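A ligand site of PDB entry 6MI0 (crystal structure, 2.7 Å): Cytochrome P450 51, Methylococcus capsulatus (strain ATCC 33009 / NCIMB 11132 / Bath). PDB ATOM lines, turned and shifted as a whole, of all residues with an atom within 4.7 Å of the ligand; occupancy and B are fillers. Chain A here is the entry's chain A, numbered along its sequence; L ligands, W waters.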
ATOM      1  N   GLN A  75     -19.089  17.973   7.015  1.00  0.00           N
ATOM      2  CA  GLN A  75     -19.628  16.820   7.783  1.00  0.00           C
ATOM      3  C   GLN A  75     -18.471  16.067   8.462  1.00  0.00           C
ATOM      4  O   GLN A  75     -18.762  15.128   9.225  1.00  0.00           O
ATOM      5  CB  GLN A  75     -20.437  15.889   6.877  1.00  0.00           C
ATOM      6  CG  GLN A  75     -19.972  15.860   5.429  1.00  0.00           C
ATOM      7  CD  GLN A  75     -20.711  14.834   4.607  1.00  0.00           C
ATOM      8  OE1 GLN A  75     -21.723  14.278   5.035  1.00  0.00           O
ATOM      9  NE2 GLN A  75     -20.225  14.590   3.399  1.00  0.00           N
ATOM     10  N   TYR A  79     -17.926  12.850  12.228  1.00  0.00           N
ATOM     11  CA  TYR A  79     -17.485  11.461  11.936  1.00  0.00           C
ATOM     12  C   TYR A  79     -16.132  11.159  12.597  1.00  0.00           C
ATOM     13  O   TYR A  79     -15.589  10.061  12.339  1.00  0.00           O
ATOM     14  CB  TYR A  79     -17.386  11.237  10.431  1.00  0.00           C
ATOM     15  CG  TYR A  79     -18.700  10.961   9.744  1.00  0.00           C
ATOM     16  CD1 TYR A  79     -19.216   9.677   9.657  1.00  0.00           C
ATOM     17  CD2 TYR A  79     -19.420  11.990   9.159  1.00  0.00           C
ATOM     18  CE1 TYR A  79     -20.419   9.423   9.014  1.00  0.00           C
ATOM     19  CE2 TYR A  79     -20.628  11.750   8.514  1.00  0.00           C
ATOM     20  CZ  TYR A  79     -21.127  10.466   8.442  1.00  0.00           C
ATOM     21  OH  TYR A  79     -22.319  10.225   7.813  1.00  0.00           O
ATOM     22  N   PHE A  92     -14.270  11.030   4.345  1.00  0.00           N
ATOM     23  CA  PHE A  92     -14.703  12.125   5.257  1.00  0.00           C
ATOM     24  C   PHE A  92     -13.545  12.673   6.095  1.00  0.00           C
ATOM     25  O   PHE A  92     -13.777  13.570   6.906  1.00  0.00           O
ATOM     26  CB  PHE A  92     -15.710  11.748   6.365  1.00  0.00           C
ATOM     27  CG  PHE A  92     -17.009  11.114   5.959  1.00  0.00           C
ATOM     28  CD1 PHE A  92     -17.978  11.841   5.311  1.00  0.00           C
ATOM     29  CD2 PHE A  92     -17.277   9.807   6.295  1.00  0.00           C
ATOM     30  CE1 PHE A  92     -19.188  11.252   4.953  1.00  0.00           C
ATOM     31  CE2 PHE A  92     -18.483   9.220   5.947  1.00  0.00           C
ATOM     32  CZ  PHE A  92     -19.437   9.944   5.280  1.00  0.00           C
ATOM     33  N   LEU A 103     -17.452   8.658  -2.499  1.00  0.00           N
ATOM     34  CA  LEU A 103     -18.931   8.649  -2.310  1.00  0.00           C
ATOM     35  C   LEU A 103     -19.621   8.363  -3.647  1.00  0.00           C
ATOM     36  O   LEU A 103     -20.578   7.556  -3.670  1.00  0.00           O
ATOM     37  CB  LEU A 103     -19.390   9.993  -1.747  1.00  0.00           C
ATOM     38  CG  LEU A 103     -18.991  10.286  -0.293  1.00  0.00           C
ATOM     39  CD1 LEU A 103     -19.539  11.624   0.154  1.00  0.00           C
ATOM     40  CD2 LEU A 103     -19.450   9.176   0.641  1.00  0.00           C
ATOM     41  N   LEU A 106     -19.723   4.822  -4.799  1.00  0.00           N
ATOM     42  CA  LEU A 106     -20.683   3.996  -4.018  1.00  0.00           C
ATOM     43  C   LEU A 106     -22.070   4.075  -4.660  1.00  0.00           C
ATOM     44  O   LEU A 106     -22.761   3.039  -4.717  1.00  0.00           O
ATOM     45  CB  LEU A 106     -20.728   4.508  -2.580  1.00  0.00           C
ATOM     46  CG  LEU A 106     -19.594   4.030  -1.677  1.00  0.00           C
ATOM     47  CD1 LEU A 106     -19.532   4.849  -0.394  1.00  0.00           C
ATOM     48  CD2 LEU A 106     -19.729   2.544  -1.358  1.00  0.00           C
ATOM     49  N   LEU A 110     -25.301   0.939  -5.223  1.00  0.00           N
ATOM     50  CA  LEU A 110     -26.437   0.841  -4.286  1.00  0.00           C
ATOM     51  C   LEU A 110     -27.761   1.190  -4.972  1.00  0.00           C
ATOM     52  O   LEU A 110     -28.796   1.207  -4.285  1.00  0.00           O
ATOM     53  CB  LEU A 110     -26.185   1.783  -3.104  1.00  0.00           C
ATOM     54  CG  LEU A 110     -24.911   1.509  -2.299  1.00  0.00           C
ATOM     55  CD1 LEU A 110     -24.622   2.658  -1.349  1.00  0.00           C
ATOM     56  CD2 LEU A 110     -25.027   0.196  -1.533  1.00  0.00           C
ATOM     57  N   LEU A 157     -22.877  -6.463  -0.040  1.00  0.00           N
ATOM     58  CA  LEU A 157     -21.859  -5.376  -0.017  1.00  0.00           C
ATOM     59  C   LEU A 157     -20.447  -5.978  -0.139  1.00  0.00           C
ATOM     60  O   LEU A 157     -19.625  -5.396  -0.859  1.00  0.00           O
ATOM     61  CB  LEU A 157     -22.004  -4.573   1.279  1.00  0.00           C
ATOM     62  CG  LEU A 157     -22.833  -3.288   1.157  1.00  0.00           C
ATOM     63  CD1 LEU A 157     -24.125  -3.547   0.398  1.00  0.00           C
ATOM     64  CD2 LEU A 157     -23.118  -2.698   2.530  1.00  0.00           C
ATOM     65  N   THR A 254     -20.154   1.942   4.639  1.00  0.00           N
ATOM     66  CA  THR A 254     -21.433   1.531   3.994  1.00  0.00           C
ATOM     67  C   THR A 254     -22.214   0.605   4.944  1.00  0.00           C
ATOM     68  O   THR A 254     -23.441   0.791   5.064  1.00  0.00           O
ATOM     69  CB  THR A 254     -21.177   0.885   2.627  1.00  0.00           C
ATOM     70  OG1 THR A 254     -20.560   1.882   1.817  1.00  0.00           O
ATOM     71  CG2 THR A 254     -22.443   0.379   1.966  1.00  0.00           C
ATOM     72  N   ALA A 257     -23.394   2.552   8.011  1.00  0.00           N
ATOM     73  CA  ALA A 257     -24.399   3.529   7.519  1.00  0.00           C
ATOM     74  C   ALA A 257     -25.761   2.840   7.374  1.00  0.00           C
ATOM     75  O   ALA A 257     -26.788   3.532   7.572  1.00  0.00           O
ATOM     76  CB  ALA A 257     -23.941   4.130   6.216  1.00  0.00           C
ATOM     77  N   GLY A 258     -25.765   1.530   7.116  1.00  0.00           N
ATOM     78  CA  GLY A 258     -26.957   0.792   6.630  1.00  0.00           C
ATOM     79  C   GLY A 258     -27.503  -0.199   7.643  1.00  0.00           C
ATOM     80  O   GLY A 258     -28.669  -0.621   7.460  1.00  0.00           O
ATOM     81  N   THR A 261     -29.680   1.395  11.134  1.00  0.00           N
ATOM     82  CA  THR A 261     -30.699   2.235  10.434  1.00  0.00           C
ATOM     83  C   THR A 261     -31.778   1.319   9.836  1.00  0.00           C
ATOM     84  O   THR A 261     -32.965   1.551  10.142  1.00  0.00           O
ATOM     85  CB  THR A 261     -30.046   3.111   9.365  1.00  0.00           C
ATOM     86  OG1 THR A 261     -29.193   2.296   8.564  1.00  0.00           O
ATOM     87  CG2 THR A 261     -29.252   4.261   9.969  1.00  0.00           C
ATOM     88  N   SER A 262     -31.384   0.318   9.044  1.00  0.00           N
ATOM     89  CA  SER A 262     -32.308  -0.663   8.412  1.00  0.00           C
ATOM     90  C   SER A 262     -32.944  -1.555   9.488  1.00  0.00           C
ATOM     91  O   SER A 262     -34.175  -1.690   9.489  1.00  0.00           O
ATOM     92  CB  SER A 262     -31.610  -1.480   7.367  1.00  0.00           C
ATOM     93  OG  SER A 262     -31.617  -0.806   6.121  1.00  0.00           O
ATOM     94  N   THR A 265     -35.525   0.107  11.696  1.00  0.00           N
ATOM     95  CA  THR A 265     -36.704   0.499  10.871  1.00  0.00           C
ATOM     96  C   THR A 265     -37.577  -0.731  10.589  1.00  0.00           C
ATOM     97  O   THR A 265     -38.811  -0.596  10.668  1.00  0.00           O
ATOM     98  CB  THR A 265     -36.258   1.179   9.577  1.00  0.00           C
ATOM     99  OG1 THR A 265     -35.716   2.450   9.940  1.00  0.00           O
ATOM    100  CG2 THR A 265     -37.384   1.357   8.589  1.00  0.00           C
ATOM    101  N   LEU A 316     -40.682   5.968   9.134  1.00  0.00           N
ATOM    102  CA  LEU A 316     -39.456   6.798   9.033  1.00  0.00           C
ATOM    103  C   LEU A 316     -39.779   8.248   9.435  1.00  0.00           C
ATOM    104  O   LEU A 316     -38.872   8.919   9.962  1.00  0.00           O
ATOM    105  CB  LEU A 316     -38.884   6.706   7.619  1.00  0.00           C
ATOM    106  CG  LEU A 316     -37.926   5.524   7.389  1.00  0.00           C
ATOM    107  CD1 LEU A 316     -37.381   5.535   5.972  1.00  0.00           C
ATOM    108  CD2 LEU A 316     -36.787   5.549   8.397  1.00  0.00           C
ATOM    109  N   PRO A 321     -34.035   6.972  12.401  1.00  0.00           N
ATOM    110  CA  PRO A 321     -32.977   6.423  13.234  1.00  0.00           C
ATOM    111  C   PRO A 321     -31.839   7.418  13.519  1.00  0.00           C
ATOM    112  O   PRO A 321     -31.171   7.244  14.521  1.00  0.00           O
ATOM    113  CB  PRO A 321     -32.445   5.230  12.425  1.00  0.00           C
ATOM    114  CG  PRO A 321     -32.839   5.532  10.995  1.00  0.00           C
ATOM    115  CD  PRO A 321     -34.143   6.294  11.103  1.00  0.00           C
ATOM    116  N   LEU A 322     -31.632   8.391  12.628  1.00  0.00           N
ATOM    117  CA  LEU A 322     -30.648   9.495  12.811  1.00  0.00           C
ATOM    118  C   LEU A 322     -31.406  10.805  13.036  1.00  0.00           C
ATOM    119  O   LEU A 322     -32.179  11.214  12.148  1.00  0.00           O
ATOM    120  CB  LEU A 322     -29.749   9.562  11.573  1.00  0.00           C
ATOM    121  CG  LEU A 322     -29.239   8.218  11.054  1.00  0.00           C
ATOM    122  CD1 LEU A 322     -28.322   8.402   9.857  1.00  0.00           C
ATOM    123  CD2 LEU A 322     -28.531   7.438  12.150  1.00  0.00           C
ATOM    124  N   LEU A 325     -28.192  15.459  12.627  1.00  0.00           N
ATOM    125  CA  LEU A 325     -27.235  15.565  11.499  1.00  0.00           C
ATOM    126  C   LEU A 325     -26.379  16.825  11.680  1.00  0.00           C
ATOM    127  O   LEU A 325     -26.887  17.926  11.361  1.00  0.00           O
ATOM    128  CB  LEU A 325     -27.997  15.639  10.170  1.00  0.00           C
ATOM    129  CG  LEU A 325     -29.147  14.640   9.994  1.00  0.00           C
ATOM    130  CD1 LEU A 325     -29.755  14.768   8.610  1.00  0.00           C
ATOM    131  CD2 LEU A 325     -28.675  13.217  10.243  1.00  0.00           C
ATOM    132  N   ARG A 327     -23.013  19.539  11.388  1.00  0.00           N
ATOM    133  CA  ARG A 327     -22.059  20.189  10.450  1.00  0.00           C
ATOM    134  C   ARG A 327     -21.295  21.294  11.183  1.00  0.00           C
ATOM    135  O   ARG A 327     -21.910  21.987  12.004  1.00  0.00           O
ATOM    136  CB  ARG A 327     -22.805  20.804   9.267  1.00  0.00           C
ATOM    137  CG  ARG A 327     -23.645  19.824   8.458  1.00  0.00           C
ATOM    138  CD  ARG A 327     -22.812  18.948   7.557  1.00  0.00           C
ATOM    139  NE  ARG A 327     -23.627  18.316   6.530  1.00  0.00           N
ATOM    140  CZ  ARG A 327     -24.325  17.197   6.693  1.00  0.00           C
ATOM    141  NH1 ARG A 327     -24.304  16.574   7.862  1.00  0.00           N
ATOM    142  NH2 ARG A 327     -25.046  16.715   5.696  1.00  0.00           N
ATOM    143  N   ALA A 386     -35.999  11.977   6.452  1.00  0.00           N
ATOM    144  CA  ALA A 386     -35.537  10.798   7.225  1.00  0.00           C
ATOM    145  C   ALA A 386     -34.211  10.299   6.638  1.00  0.00           C
ATOM    146  O   ALA A 386     -33.408   9.740   7.402  1.00  0.00           O
ATOM    147  CB  ALA A 386     -36.596   9.718   7.208  1.00  0.00           C
ATOM    148  N   PHE A 387     -34.002  10.513   5.341  1.00  0.00           N
ATOM    149  CA  PHE A 387     -32.808  10.079   4.572  1.00  0.00           C
ATOM    150  C   PHE A 387     -31.857  11.257   4.352  1.00  0.00           C
ATOM    151  O   PHE A 387     -31.018  11.200   3.428  1.00  0.00           O
ATOM    152  CB  PHE A 387     -33.211   9.511   3.205  1.00  0.00           C
ATOM    153  CG  PHE A 387     -33.774   8.114   3.239  1.00  0.00           C
ATOM    154  CD1 PHE A 387     -33.090   7.098   3.873  1.00  0.00           C
ATOM    155  CD2 PHE A 387     -34.967   7.827   2.611  1.00  0.00           C
ATOM    156  CE1 PHE A 387     -33.599   5.810   3.886  1.00  0.00           C
ATOM    157  CE2 PHE A 387     -35.487   6.536   2.631  1.00  0.00           C
ATOM    158  CZ  PHE A 387     -34.795   5.530   3.269  1.00  0.00           C
ATOM    159  N   GLY A 388     -32.000  12.316   5.158  1.00  0.00           N
ATOM    160  CA  GLY A 388     -31.322  13.604   4.937  1.00  0.00           C
ATOM    161  C   GLY A 388     -31.769  14.230   3.631  1.00  0.00           C
ATOM    162  O   GLY A 388     -32.919  13.970   3.226  1.00  0.00           O
ATOM    163  N   HIS A 392     -25.493  15.380  -0.079  1.00  0.00           N
ATOM    164  CA  HIS A 392     -24.997  14.309   0.831  1.00  0.00           C
ATOM    165  C   HIS A 392     -26.170  13.541   1.449  1.00  0.00           C
ATOM    166  O   HIS A 392     -26.031  13.044   2.585  1.00  0.00           O
ATOM    167  CB  HIS A 392     -24.061  14.906   1.888  1.00  0.00           C
ATOM    168  CG  HIS A 392     -22.750  15.328   1.329  1.00  0.00           C
ATOM    169  ND1 HIS A 392     -21.948  14.456   0.614  1.00  0.00           N
ATOM    170  CD2 HIS A 392     -22.111  16.515   1.337  1.00  0.00           C
ATOM    171  CE1 HIS A 392     -20.857  15.083   0.232  1.00  0.00           C
ATOM    172  NE2 HIS A 392     -20.935  16.355   0.665  1.00  0.00           N
ATOM    173  N   LYS A 393     -27.261  13.404   0.698  1.00  0.00           N
ATOM    174  CA  LYS A 393     -28.412  12.521   1.006  1.00  0.00           C
ATOM    175  C   LYS A 393     -27.957  11.060   0.874  1.00  0.00           C
ATOM    176  O   LYS A 393     -26.990  10.801   0.135  1.00  0.00           O
ATOM    177  CB  LYS A 393     -29.569  12.889   0.074  1.00  0.00           C
ATOM    178  CG  LYS A 393     -30.558  11.779  -0.254  1.00  0.00           C
ATOM    179  CD  LYS A 393     -31.879  12.319  -0.752  1.00  0.00           C
ATOM    180  CE  LYS A 393     -33.016  11.322  -0.604  1.00  0.00           C
ATOM    181  NZ  LYS A 393     -34.153  11.671  -1.483  1.00  0.00           N
ATOM    182  N   CYS A 394     -28.602  10.153   1.628  1.00  0.00           N
ATOM    183  CA  CYS A 394     -28.330   8.691   1.665  1.00  0.00           C
ATOM    184  C   CYS A 394     -28.136   8.161   0.240  1.00  0.00           C
ATOM    185  O   CYS A 394     -28.994   8.442  -0.618  1.00  0.00           O
ATOM    186  CB  CYS A 394     -29.493   7.986   2.353  1.00  0.00           C
ATOM    187  SG  CYS A 394     -29.117   6.304   2.923  1.00  0.00           S
ATOM    188  N   SER A 395     -27.038   7.431  -0.005  1.00  0.00           N
ATOM    189  CA  SER A 395     -26.734   6.764  -1.299  1.00  0.00           C
ATOM    190  C   SER A 395     -27.580   5.496  -1.436  1.00  0.00           C
ATOM    191  O   SER A 395     -27.809   5.050  -2.589  1.00  0.00           O
ATOM    192  CB  SER A 395     -25.268   6.431  -1.426  1.00  0.00           C
ATOM    193  OG  SER A 395     -24.452   7.576  -1.173  1.00  0.00           O
ATOM    194  N   GLY A 396     -28.009   4.937  -0.296  1.00  0.00           N
ATOM    195  CA  GLY A 396     -28.636   3.611  -0.215  1.00  0.00           C
ATOM    196  C   GLY A 396     -30.052   3.672   0.336  1.00  0.00           C
ATOM    197  O   GLY A 396     -30.470   2.688   0.967  1.00  0.00           O
ATOM    198  N   PHE A 399     -31.598   0.936  -1.736  1.00  0.00           N
ATOM    199  CA  PHE A 399     -31.188  -0.360  -1.136  1.00  0.00           C
ATOM    200  C   PHE A 399     -32.033  -0.641   0.119  1.00  0.00           C
ATOM    201  O   PHE A 399     -32.608  -1.734   0.216  1.00  0.00           O
ATOM    202  CB  PHE A 399     -29.707  -0.375  -0.784  1.00  0.00           C
ATOM    203  CG  PHE A 399     -29.216  -1.717  -0.291  1.00  0.00           C
ATOM    204  CD1 PHE A 399     -28.834  -2.701  -1.185  1.00  0.00           C
ATOM    205  CD2 PHE A 399     -29.229  -2.019   1.061  1.00  0.00           C
ATOM    206  CE1 PHE A 399     -28.432  -3.944  -0.733  1.00  0.00           C
ATOM    207  CE2 PHE A 399     -28.827  -3.263   1.513  1.00  0.00           C
ATOM    208  CZ  PHE A 399     -28.423  -4.223   0.613  1.00  0.00           C
ATOM    209  N   ALA A 400     -32.068   0.324   1.046  1.00  0.00           N
ATOM    210  CA  ALA A 400     -32.798   0.255   2.327  1.00  0.00           C
ATOM    211  C   ALA A 400     -34.267  -0.134   2.076  1.00  0.00           C
ATOM    212  O   ALA A 400     -34.771  -1.031   2.771  1.00  0.00           O
ATOM    213  CB  ALA A 400     -32.703   1.584   3.039  1.00  0.00           C
ATOM    214  N   GLN A 403     -34.464  -3.791   0.794  1.00  0.00           N
ATOM    215  CA  GLN A 403     -34.036  -4.634   1.940  1.00  0.00           C
ATOM    216  C   GLN A 403     -35.235  -4.840   2.867  1.00  0.00           C
ATOM    217  O   GLN A 403     -35.575  -6.005   3.144  1.00  0.00           O
ATOM    218  CB  GLN A 403     -32.838  -4.004   2.657  1.00  0.00           C
ATOM    219  CG  GLN A 403     -32.370  -4.812   3.865  1.00  0.00           C
ATOM    220  CD  GLN A 403     -30.943  -4.534   4.246  1.00  0.00           C
ATOM    221  OE1 GLN A 403     -30.097  -5.436   4.247  1.00  0.00           O
ATOM    222  NE2 GLN A 403     -30.661  -3.300   4.607  1.00  0.00           N
ATOM    223  N   ILE A 404     -35.913  -3.743   3.259  1.00  0.00           N
ATOM    224  CA  ILE A 404     -36.997  -3.762   4.287  1.00  0.00           C
ATOM    225  C   ILE A 404     -38.263  -4.369   3.687  1.00  0.00           C
ATOM    226  O   ILE A 404     -38.917  -5.154   4.391  1.00  0.00           O
ATOM    227  CB  ILE A 404     -37.240  -2.351   4.854  1.00  0.00           C
ATOM    228  CG1 ILE A 404     -35.941  -1.723   5.375  1.00  0.00           C
ATOM    229  CG2 ILE A 404     -38.317  -2.392   5.941  1.00  0.00           C
ATOM    230  CD1 ILE A 404     -36.055  -0.255   5.694  1.00  0.00           C
HETATM  231  C1  LIG L   1     -26.224   8.882   4.787  1.00  0.00           C
HETATM  232  C2  LIG L   1     -30.474   7.806   6.807  1.00  0.00           C
HETATM  233  C3  LIG L   1     -30.012   3.187   5.280  1.00  0.00           C
HETATM  234  C4  LIG L   1     -25.810   4.330   3.185  1.00  0.00           C
HETATM  235  C5  LIG L   1     -27.419   8.960   5.467  1.00  0.00           C
HETATM  236  C6  LIG L   1     -27.913  10.148   6.043  1.00  0.00           C
HETATM  237  C7  LIG L   1     -29.106   9.854   6.602  1.00  0.00           C
HETATM  238  C8  LIG L   1     -29.350   8.488   6.395  1.00  0.00           C
HETATM  239  C9  LIG L   1     -29.999  10.829   7.334  1.00  0.00           C
HETATM  240  C10 LIG L   1     -27.251  11.514   6.003  1.00  0.00           C
HETATM  241  C11 LIG L   1     -26.424  11.799   7.253  1.00  0.00           C
HETATM  242  C12 LIG L   1     -25.903  13.210   7.212  1.00  0.00           C
HETATM  243  O1  LIG L   1     -26.409  14.063   6.456  1.00  0.00           O
HETATM  244  O2  LIG L   1     -24.939  13.534   7.952  1.00  0.00           O
HETATM  245  C13 LIG L   1     -30.680   6.441   6.535  1.00  0.00           C
HETATM  246  C14 LIG L   1     -31.848   5.783   6.986  1.00  0.00           C
HETATM  247  C15 LIG L   1     -31.760   4.488   6.588  1.00  0.00           C
HETATM  248  C16 LIG L   1     -30.469   4.374   5.860  1.00  0.00           C
HETATM  249  C17 LIG L   1     -32.971   6.397   7.775  1.00  0.00           C
HETATM  250  C18 LIG L   1     -32.801   3.477   6.865  1.00  0.00           C
HETATM  251  C19 LIG L   1     -32.705   2.233   6.404  1.00  0.00           C
HETATM  252  C20 LIG L   1     -28.821   3.097   4.571  1.00  0.00           C
HETATM  253  C21 LIG L   1     -28.344   1.943   3.926  1.00  0.00           C
HETATM  254  C22 LIG L   1     -27.131   2.279   3.323  1.00  0.00           C
HETATM  255  C23 LIG L   1     -26.904   3.646   3.618  1.00  0.00           C
HETATM  256  C24 LIG L   1     -29.014   0.599   3.906  1.00  0.00           C
HETATM  257  C25 LIG L   1     -26.209   1.417   2.558  1.00  0.00           C
HETATM  258  C26 LIG L   1     -26.376   0.105   2.459  1.00  0.00           C
HETATM  259  C27 LIG L   1     -25.619   5.676   3.481  1.00  0.00           C
HETATM  260  C28 LIG L   1     -24.425   6.388   3.016  1.00  0.00           C
HETATM  261  C29 LIG L   1     -24.548   7.658   3.459  1.00  0.00           C
HETATM  262  C30 LIG L   1     -25.809   7.709   4.201  1.00  0.00           C
HETATM  263  C31 LIG L   1     -23.302   5.816   2.192  1.00  0.00           C
HETATM  264  C32 LIG L   1     -23.581   8.791   3.255  1.00  0.00           C
HETATM  265  C33 LIG L   1     -24.107   9.740   2.175  1.00  0.00           C
HETATM  266  C34 LIG L   1     -23.241  10.956   2.065  1.00  0.00           C
HETATM  267  O3  LIG L   1     -22.850  11.366   0.948  1.00  0.00           O
HETATM  268  O4  LIG L   1     -22.904  11.584   3.095  1.00  0.00           O
HETATM  269  N1  LIG L   1     -28.307   7.941   5.683  1.00  0.00           N
HETATM  270  N2  LIG L   1     -29.890   5.584   5.868  1.00  0.00           N
HETATM  271  N3  LIG L   1     -27.942   4.114   4.370  1.00  0.00           N
HETATM  272  N4  LIG L   1     -26.414   6.504   4.181  1.00  0.00           N
HETATM  273 FE1  LIG L   1     -28.046   6.104   4.992  1.00  0.00          FE
HETATM  274  O   HOH W   1     -28.024  15.056   4.257  1.00  0.00           O
HETATM  275  O   HOH W   2     -23.197  10.679  -1.475  1.00  0.00           O
HETATM  276  O   HOH W   3     -27.225   6.041   7.476  1.00  0.00           O
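A nitrogen (N3) of the ligand lies close to the backbone carbonyl oxygen (O) of Ala 257 (3.5 Å). OE1 of Gln 75 touches O4 of the ligand (3.5 Å). Leu 103 touches the ligand (CD1 to O3, 3.4 Å). Thr 254 touches the ligand. Gly 258 touches the ligand. Thr 261 touches the ligand. Ser 262 touches the ligand (OG to C19, 3.2 Å). CD2 of Leu 316 touches C17 of the ligand, at 3.96 Å. Pro 321 touches the ligand (CG to C17, 3.3 Å). Leu 322 touches the ligand (CD1 to C8, 3.6 Å). Leu 325 touches the ligand. Ala 386 touches the ligand. CE1 of Phe 387 touches C15 of the ligand, 3.5 Å away. N of Gly 388 touches C9 of the ligand (3.3 Å). Lys 393 touches the ligand. Ser 395 touches the ligand (OG to C31, 3.97 Å). Gly 396 touches the ligand. Phe 399 touches the ligand. CB of Ala 400 touches C19 of the ligand (3.4 Å). Hydrophobic or aromatic side chains that line the ligand: Leu 103, Ala 257, Leu 316, Pro 321, Leu 322, Leu 325, Phe 387, His 392, Phe 399 and Ala 400.
The side-chain sulfur (SG) of Cys 394 binds an iron atom (FE1) of the ligand (2.3 Å). NH2 of Arg 327 is in salt-bridge range of O1 of the ligand (3.1 Å). A ring nitrogen (ND1) of His 392 lies within hydrogen-bond range of an oxygen (O3) of the ligand (3.2 Å).
Water W2 bridges an oxygen (O3) of the ligand and the side-chain hydroxyl of Ser 395. Water W1 lies within hydrogen-bond range of an oxygen (O1) of the ligand and the backbone carbonyl oxygen (O) of His 392.
N of Cys 394 lies within hydrogen-bond range of O of Phe 387 (3.2 Å). N of Gly 396 sits close to SG of Cys 394. The side-chain amide nitrogen (NE2) of Gln 75 sits close to a ring nitrogen (ND1) of His 392 (3.3 Å). The side-chain hydroxyl of Ser 262 sits close to the backbone carbonyl oxygen of Gly 258. The side-chain hydroxyl of Ser 262 lies within hydrogen-bond range of the side-chain amide nitrogen of Gln 403, at 3.1 Å. O of Gly 258 sits close to OG1 of Thr 261 (3.2 Å). O of Ala 257 is in hydrogen-bond range of OG1 of Thr 261, 2.9 Å away. O of Thr 261 sits at hydrogen-bond distance from OG1 of Thr 265.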
